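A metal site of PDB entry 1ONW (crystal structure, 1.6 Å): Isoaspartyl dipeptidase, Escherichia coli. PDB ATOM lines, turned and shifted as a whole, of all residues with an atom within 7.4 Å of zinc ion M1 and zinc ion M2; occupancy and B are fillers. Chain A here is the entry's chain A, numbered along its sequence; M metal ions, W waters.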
ATOM      1  N   HIS A  68      -0.330  23.505 -15.815  1.00  0.00           N
ATOM      2  CA  HIS A  68      -1.323  23.634 -14.766  1.00  0.00           C
ATOM      3  C   HIS A  68      -2.258  22.460 -14.777  1.00  0.00           C
ATOM      4  O   HIS A  68      -3.329  22.510 -15.381  1.00  0.00           O
ATOM      5  CB  HIS A  68      -2.093  24.956 -14.912  1.00  0.00           C
ATOM      6  CG  HIS A  68      -2.961  25.303 -13.724  1.00  0.00           C
ATOM      7  ND1 HIS A  68      -2.845  26.545 -13.106  1.00  0.00           N
ATOM      8  CD2 HIS A  68      -3.951  24.614 -13.103  1.00  0.00           C
ATOM      9  CE1 HIS A  68      -3.733  26.607 -12.128  1.00  0.00           C
ATOM     10  NE2 HIS A  68      -4.379  25.453 -12.109  1.00  0.00           N
ATOM     11  N   VAL A  69      -1.824  21.377 -14.133  1.00  0.00           N
ATOM     12  CA  VAL A  69      -2.612  20.162 -14.063  1.00  0.00           C
ATOM     13  C   VAL A  69      -2.780  19.674 -12.623  1.00  0.00           C
ATOM     14  O   VAL A  69      -1.834  19.610 -11.858  1.00  0.00           O
ATOM     15  CB  VAL A  69      -1.927  19.050 -14.879  1.00  0.00           C
ATOM     16  CG1 VAL A  69      -2.859  17.831 -15.009  1.00  0.00           C
ATOM     17  CG2 VAL A  69      -1.545  19.570 -16.267  1.00  0.00           C
ATOM     18  N   HIS A  70      -4.000  19.264 -12.266  1.00  0.00           N
ATOM     19  CA  HIS A  70      -4.232  18.711 -10.924  1.00  0.00           C
ATOM     20  C   HIS A  70      -3.972  17.201 -11.006  1.00  0.00           C
ATOM     21  O   HIS A  70      -4.870  16.338 -11.006  1.00  0.00           O
ATOM     22  CB  HIS A  70      -5.656  19.057 -10.445  1.00  0.00           C
ATOM     23  CG  HIS A  70      -5.754  20.525 -10.267  1.00  0.00           C
ATOM     24  ND1 HIS A  70      -5.504  21.146  -9.037  1.00  0.00           N
ATOM     25  CD2 HIS A  70      -5.998  21.494 -11.189  1.00  0.00           C
ATOM     26  CE1 HIS A  70      -5.649  22.459  -9.226  1.00  0.00           C
ATOM     27  NE2 HIS A  70      -5.932  22.684 -10.500  1.00  0.00           N
ATOM     28  N   LEU A 103      -0.048  20.655  -9.680  1.00  0.00           N
ATOM     29  CA  LEU A 103      -0.226  21.579  -8.577  1.00  0.00           C
ATOM     30  C   LEU A 103      -1.490  21.195  -7.814  1.00  0.00           C
ATOM     31  O   LEU A 103      -2.254  20.326  -8.233  1.00  0.00           O
ATOM     32  CB  LEU A 103      -0.249  23.078  -9.023  1.00  0.00           C
ATOM     33  CG  LEU A 103      -1.028  23.334 -10.312  1.00  0.00           C
ATOM     34  CD1 LEU A 103      -2.500  23.069 -10.070  1.00  0.00           C
ATOM     35  CD2 LEU A 103      -0.874  24.785 -10.774  1.00  0.00           C
ATOM     36  N   LEU A 104      -1.675  21.899  -6.702  1.00  0.00           N
ATOM     37  CA  LEU A 104      -2.849  21.754  -5.840  1.00  0.00           C
ATOM     38  C   LEU A 104      -3.673  23.048  -5.908  1.00  0.00           C
ATOM     39  O   LEU A 104      -3.151  24.089  -6.332  1.00  0.00           O
ATOM     40  CB  LEU A 104      -2.459  21.504  -4.357  1.00  0.00           C
ATOM     41  CG  LEU A 104      -1.567  20.284  -4.089  1.00  0.00           C
ATOM     42  CD1 LEU A 104      -1.355  20.155  -2.573  1.00  0.00           C
ATOM     43  CD2 LEU A 104      -2.287  19.021  -4.583  1.00  0.00           C
ATOM     44  N   GLY A 105      -4.908  23.022  -5.433  1.00  0.00           N
ATOM     45  CA  GLY A 105      -5.762  24.203  -5.489  1.00  0.00           C
ATOM     46  C   GLY A 105      -6.405  24.531  -4.160  1.00  0.00           C
ATOM     47  O   GLY A 105      -5.733  24.776  -3.155  1.00  0.00           O
ATOM     48  N   THR A 106      -7.726  24.659  -4.200  1.00  0.00           N
ATOM     49  CA  THR A 106      -8.492  25.005  -3.025  1.00  0.00           C
ATOM     50  C   THR A 106      -8.189  24.073  -1.850  1.00  0.00           C
ATOM     51  O   THR A 106      -7.911  24.511  -0.740  1.00  0.00           O
ATOM     52  CB  THR A 106      -9.987  24.962  -3.330  1.00  0.00           C
ATOM     53  OG1 THR A 106     -10.194  25.739  -4.488  1.00  0.00           O
ATOM     54  CG2 THR A 106     -10.731  25.580  -2.182  1.00  0.00           C
ATOM     55  N   TYR A 137      -3.789  26.792  -2.846  1.00  0.00           N
ATOM     56  CA  TYR A 137      -4.317  28.158  -2.699  1.00  0.00           C
ATOM     57  C   TYR A 137      -3.877  28.743  -1.376  1.00  0.00           C
ATOM     58  O   TYR A 137      -3.656  29.950  -1.258  1.00  0.00           O
ATOM     59  CB  TYR A 137      -5.863  28.251  -2.649  1.00  0.00           C
ATOM     60  CG  TYR A 137      -6.631  28.052  -3.953  1.00  0.00           C
ATOM     61  CD1 TYR A 137      -6.049  27.508  -5.088  1.00  0.00           C
ATOM     62  CD2 TYR A 137      -7.980  28.425  -3.998  1.00  0.00           C
ATOM     63  CE1 TYR A 137      -6.794  27.313  -6.256  1.00  0.00           C
ATOM     64  CE2 TYR A 137      -8.742  28.240  -5.156  1.00  0.00           C
ATOM     65  CZ  TYR A 137      -8.141  27.681  -6.284  1.00  0.00           C
ATOM     66  OH  TYR A 137      -8.878  27.460  -7.413  1.00  0.00           O
ATOM     67  N   KCX A 162       2.611  27.703  -5.595  1.00  0.00           N
ATOM     68  CA  KCX A 162       1.274  28.041  -6.020  1.00  0.00           C
ATOM     69  CB  KCX A 162       0.469  26.742  -6.267  1.00  0.00           C
ATOM     70  CG  KCX A 162      -1.037  26.955  -6.391  1.00  0.00           C
ATOM     71  CD  KCX A 162      -1.397  27.653  -7.704  1.00  0.00           C
ATOM     72  CE  KCX A 162      -2.897  27.780  -7.938  1.00  0.00           C
ATOM     73  NZ  KCX A 162      -3.468  26.452  -8.162  1.00  0.00           N
ATOM     74  C   KCX A 162       0.576  28.824  -4.904  1.00  0.00           C
ATOM     75  O   KCX A 162       0.929  28.683  -3.714  1.00  0.00           O
ATOM     76  CX  KCX A 162      -4.618  26.585  -9.011  1.00  0.00           C
ATOM     77  OQ1 KCX A 162      -4.920  27.623  -9.575  1.00  0.00           O
ATOM     78  OQ2 KCX A 162      -5.265  25.462  -9.111  1.00  0.00           O
ATOM     79  N   CYS A 163      -0.406  29.654  -5.267  1.00  0.00           N
ATOM     80  CA  CYS A 163      -1.208  30.430  -4.325  1.00  0.00           C
ATOM     81  C   CYS A 163      -2.494  30.915  -5.002  1.00  0.00           C
ATOM     82  O   CYS A 163      -2.669  30.792  -6.194  1.00  0.00           O
ATOM     83  CB  CYS A 163      -0.441  31.600  -3.673  1.00  0.00           C
ATOM     84  SG  CYS A 163      -0.247  33.091  -4.709  1.00  0.00           S
ATOM     85  N   ALA A 164      -3.401  31.469  -4.220  1.00  0.00           N
ATOM     86  CA  ALA A 164      -4.631  32.036  -4.753  1.00  0.00           C
ATOM     87  C   ALA A 164      -4.772  33.446  -4.213  1.00  0.00           C
ATOM     88  O   ALA A 164      -4.534  33.701  -3.033  1.00  0.00           O
ATOM     89  CB  ALA A 164      -5.870  31.257  -4.339  1.00  0.00           C
ATOM     90  N   ASP A 167      -9.735  35.999  -4.781  1.00  0.00           N
ATOM     91  CA  ASP A 167     -10.666  34.912  -4.969  1.00  0.00           C
ATOM     92  C   ASP A 167     -11.373  34.576  -3.659  1.00  0.00           C
ATOM     93  O   ASP A 167     -10.737  34.552  -2.613  1.00  0.00           O
ATOM     94  CB  ASP A 167      -9.879  33.701  -5.487  1.00  0.00           C
ATOM     95  CG  ASP A 167     -10.782  32.536  -5.750  1.00  0.00           C
ATOM     96  OD1 ASP A 167     -11.232  31.775  -4.908  1.00  0.00           O
ATOM     97  OD2 ASP A 167     -11.010  32.407  -7.008  1.00  0.00           O
ATOM     98  N   ARG A 169     -12.051  31.978  -2.422  1.00  0.00           N
ATOM     99  CA  ARG A 169     -11.507  30.758  -1.806  1.00  0.00           C
ATOM    100  C   ARG A 169     -10.079  30.944  -1.345  1.00  0.00           C
ATOM    101  O   ARG A 169      -9.408  29.965  -1.045  1.00  0.00           O
ATOM    102  CB  ARG A 169     -11.551  29.534  -2.709  1.00  0.00           C
ATOM    103  CG  ARG A 169     -12.945  29.075  -3.072  1.00  0.00           C
ATOM    104  CD  ARG A 169     -12.956  28.387  -4.437  1.00  0.00           C
ATOM    105  NE  ARG A 169     -12.553  29.319  -5.489  1.00  0.00           N
ATOM    106  CZ  ARG A 169     -12.471  29.002  -6.782  1.00  0.00           C
ATOM    107  NH1 ARG A 169     -12.740  27.781  -7.245  1.00  0.00           N
ATOM    108  NH2 ARG A 169     -12.091  29.935  -7.646  1.00  0.00           N
ATOM    109  N   PHE A 200      -0.105  32.499  -9.561  1.00  0.00           N
ATOM    110  CA  PHE A 200      -1.260  33.022  -8.894  1.00  0.00           C
ATOM    111  C   PHE A 200      -2.605  32.635  -9.473  1.00  0.00           C
ATOM    112  O   PHE A 200      -2.980  33.088 -10.557  1.00  0.00           O
ATOM    113  CB  PHE A 200      -1.240  34.546  -8.933  1.00  0.00           C
ATOM    114  CG  PHE A 200      -0.019  35.108  -8.302  1.00  0.00           C
ATOM    115  CD1 PHE A 200       1.160  35.205  -9.040  1.00  0.00           C
ATOM    116  CD2 PHE A 200      -0.060  35.565  -6.986  1.00  0.00           C
ATOM    117  CE1 PHE A 200       2.295  35.750  -8.450  1.00  0.00           C
ATOM    118  CE2 PHE A 200       1.074  36.116  -6.384  1.00  0.00           C
ATOM    119  CZ  PHE A 200       2.252  36.222  -7.125  1.00  0.00           C
ATOM    120  N   HIS A 201      -3.356  31.821  -8.739  1.00  0.00           N
ATOM    121  CA  HIS A 201      -4.679  31.469  -9.187  1.00  0.00           C
ATOM    122  C   HIS A 201      -5.445  32.746  -8.997  1.00  0.00           C
ATOM    123  O   HIS A 201      -5.446  33.285  -7.893  1.00  0.00           O
ATOM    124  CB  HIS A 201      -5.330  30.400  -8.292  1.00  0.00           C
ATOM    125  CG  HIS A 201      -6.823  30.447  -8.367  1.00  0.00           C
ATOM    126  ND1 HIS A 201      -7.553  29.595  -9.193  1.00  0.00           N
ATOM    127  CD2 HIS A 201      -7.710  31.251  -7.725  1.00  0.00           C
ATOM    128  CE1 HIS A 201      -8.837  29.870  -9.047  1.00  0.00           C
ATOM    129  NE2 HIS A 201      -8.973  30.862  -8.166  1.00  0.00           N
ATOM    130  N   MET A 202      -6.036  33.260 -10.063  1.00  0.00           N
ATOM    131  CA  MET A 202      -6.804  34.488  -9.968  1.00  0.00           C
ATOM    132  C   MET A 202      -8.292  34.171  -9.819  1.00  0.00           C
ATOM    133  O   MET A 202      -8.787  33.263 -10.490  1.00  0.00           O
ATOM    134  CB  MET A 202      -6.654  35.390 -11.211  1.00  0.00           C
ATOM    135  CG  MET A 202      -5.214  35.715 -11.508  1.00  0.00           C
ATOM    136  SD  MET A 202      -4.379  36.579 -10.154  1.00  0.00           S
ATOM    137  CE  MET A 202      -5.569  37.916  -9.784  1.00  0.00           C
ATOM    138  N   THR A 229      -2.674  33.309 -13.482  1.00  0.00           N
ATOM    139  CA  THR A 229      -3.332  32.327 -14.348  1.00  0.00           C
ATOM    140  C   THR A 229      -4.829  32.519 -14.304  1.00  0.00           C
ATOM    141  O   THR A 229      -5.316  33.238 -13.409  1.00  0.00           O
ATOM    142  CB  THR A 229      -2.824  30.875 -14.106  1.00  0.00           C
ATOM    143  OG1 THR A 229      -3.372  30.035 -15.107  1.00  0.00           O
ATOM    144  CG2 THR A 229      -3.114  30.371 -12.684  1.00  0.00           C
ATOM    145  N   HIS A 230      -5.569  31.954 -15.263  1.00  0.00           N
ATOM    146  CA  HIS A 230      -7.021  32.137 -15.328  1.00  0.00           C
ATOM    147  C   HIS A 230      -7.311  33.582 -15.706  1.00  0.00           C
ATOM    148  O   HIS A 230      -8.352  34.143 -15.385  1.00  0.00           O
ATOM    149  CB  HIS A 230      -7.716  31.887 -13.975  1.00  0.00           C
ATOM    150  CG  HIS A 230      -7.336  30.592 -13.357  1.00  0.00           C
ATOM    151  ND1 HIS A 230      -7.170  29.450 -14.105  1.00  0.00           N
ATOM    152  CD2 HIS A 230      -7.123  30.271 -12.055  1.00  0.00           C
ATOM    153  CE1 HIS A 230      -6.858  28.471 -13.283  1.00  0.00           C
ATOM    154  NE2 HIS A 230      -6.819  28.940 -12.046  1.00  0.00           N
ATOM    155  N   ARG A 233     -10.669  34.698 -17.210  1.00  0.00           N
ATOM    156  CA  ARG A 233     -11.860  34.442 -16.419  1.00  0.00           C
ATOM    157  C   ARG A 233     -12.824  35.608 -16.327  1.00  0.00           C
ATOM    158  O   ARG A 233     -14.024  35.421 -16.093  1.00  0.00           O
ATOM    159  CB  ARG A 233     -11.507  33.886 -15.047  1.00  0.00           C
ATOM    160  CG  ARG A 233     -11.001  34.953 -14.089  1.00  0.00           C
ATOM    161  CD  ARG A 233     -10.835  34.430 -12.680  1.00  0.00           C
ATOM    162  NE  ARG A 233     -12.003  33.653 -12.280  1.00  0.00           N
ATOM    163  CZ  ARG A 233     -12.015  32.379 -11.913  1.00  0.00           C
ATOM    164  NH1 ARG A 233     -10.909  31.632 -11.791  1.00  0.00           N
ATOM    165  NH2 ARG A 233     -13.189  31.851 -11.609  1.00  0.00           N
ATOM    166  N   THR A 254      -6.197  30.158 -19.489  1.00  0.00           N
ATOM    167  CA  THR A 254      -6.685  28.796 -19.259  1.00  0.00           C
ATOM    168  C   THR A 254      -7.549  28.271 -20.403  1.00  0.00           C
ATOM    169  O   THR A 254      -8.586  28.825 -20.699  1.00  0.00           O
ATOM    170  CB  THR A 254      -7.392  28.696 -17.881  1.00  0.00           C
ATOM    171  OG1 THR A 254      -6.547  29.226 -16.883  1.00  0.00           O
ATOM    172  CG2 THR A 254      -7.762  27.250 -17.577  1.00  0.00           C
ATOM    173  N   SER A 284      -4.145  23.995 -19.134  1.00  0.00           N
ATOM    174  CA  SER A 284      -5.503  23.475 -19.170  1.00  0.00           C
ATOM    175  C   SER A 284      -6.295  23.553 -17.900  1.00  0.00           C
ATOM    176  O   SER A 284      -7.529  23.623 -17.947  1.00  0.00           O
ATOM    177  CB  SER A 284      -5.453  21.993 -19.578  1.00  0.00           C
ATOM    178  OG  SER A 284      -4.752  21.237 -18.584  1.00  0.00           O
ATOM    179  N   ASP A 285      -5.611  23.443 -16.767  1.00  0.00           N
ATOM    180  CA  ASP A 285      -6.296  23.346 -15.481  1.00  0.00           C
ATOM    181  C   ASP A 285      -7.015  21.984 -15.437  1.00  0.00           C
ATOM    182  O   ASP A 285      -8.048  21.795 -14.782  1.00  0.00           O
ATOM    183  CB  ASP A 285      -7.257  24.477 -15.140  1.00  0.00           C
ATOM    184  CG  ASP A 285      -7.453  24.497 -13.653  1.00  0.00           C
ATOM    185  OD1 ASP A 285      -6.781  23.818 -12.923  1.00  0.00           O
ATOM    186  OD2 ASP A 285      -8.412  25.293 -13.237  1.00  0.00           O
ATOM    187  N   GLY A 286      -6.444  21.039 -16.175  1.00  0.00           N
ATOM    188  CA  GLY A 286      -6.965  19.705 -16.335  1.00  0.00           C
ATOM    189  C   GLY A 286      -7.012  18.898 -15.057  1.00  0.00           C
ATOM    190  O   GLY A 286      -6.178  19.012 -14.158  1.00  0.00           O
ATOM    191  N   GLY A 288      -9.134  19.134 -12.893  1.00  0.00           N
ATOM    192  CA  GLY A 288      -9.784  19.821 -11.830  1.00  0.00           C
ATOM    193  C   GLY A 288     -11.281  19.498 -11.945  1.00  0.00           C
ATOM    194  O   GLY A 288     -11.693  18.635 -12.752  1.00  0.00           O
HETATM  195 ZN    ZN M   1      -6.007  24.734 -10.886  1.00  0.00          ZN
HETATM  196 ZN    ZN M   2      -6.923  27.919 -10.203  1.00  0.00          ZN
HETATM  197  O   HOH W   1      -7.741  25.840 -10.432  1.00  0.00           O
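NH2 of Arg 169 lies within hydrogen-bond range of NE2 of His 201, 3.3 Å away. NZ of KCX 162 lies within hydrogen-bond range of the backbone carbonyl oxygen (O) of Leu 104. A ring nitrogen (ND1) of His 70 lies within hydrogen-bond range of the backbone carbonyl oxygen (O) of Leu 103 (3.4 Å). The backbone carbonyl oxygen (O) of Gly 286 sits at hydrogen-bond distance from the backbone NH (N) of His 70 (2.9 Å). A ring nitrogen (ND1) of His 230 sits at hydrogen-bond distance from the side-chain hydroxyl (OG1) of Thr 254 (2.9 Å). N of Tyr 137 sits at hydrogen-bond distance from O of Gly 105. The backbone carbonyl oxygen of Tyr 137 is in hydrogen-bond range of the backbone NH of Ala 164, at 3.3 Å. The backbone carbonyl oxygen (O) of Val 69 lies within hydrogen-bond range of the backbone NH (N) of Leu 103 (3.0 Å).
Leu 103 touches zinc ion M1 (CD1 to ZN, 3.97 Å).
OH of Tyr 137 touches zinc ion M2, 3.4 Å away. Along chain A the residues within 4 Å of zinc ion M2 span positions 68 to 230. The nearest printed residue that does not touch zinc ion M2 is Asp 285 (4.3 Å).
Zinc ion M1 is bound by OQ2 of KCX 162 (2.1 Å), NE2 of His 70 (2.1 Å), water W1 (2.1 Å), NE2 of His 68 (2.2 Å) and OD1 of Asp 285 (2.4 Å).
ND1 of His 201 binds zinc ion M2 (2.1 Å). A ring nitrogen (NE2) of His 230 is bound to zinc ion M2. Zinc ion M2 is bound by OQ1 of KCX 162 (2.1 Å). Water W1 is bound to zinc ion M2 (2.2 Å). Zinc ion M2 has four donor atoms within binding distance.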
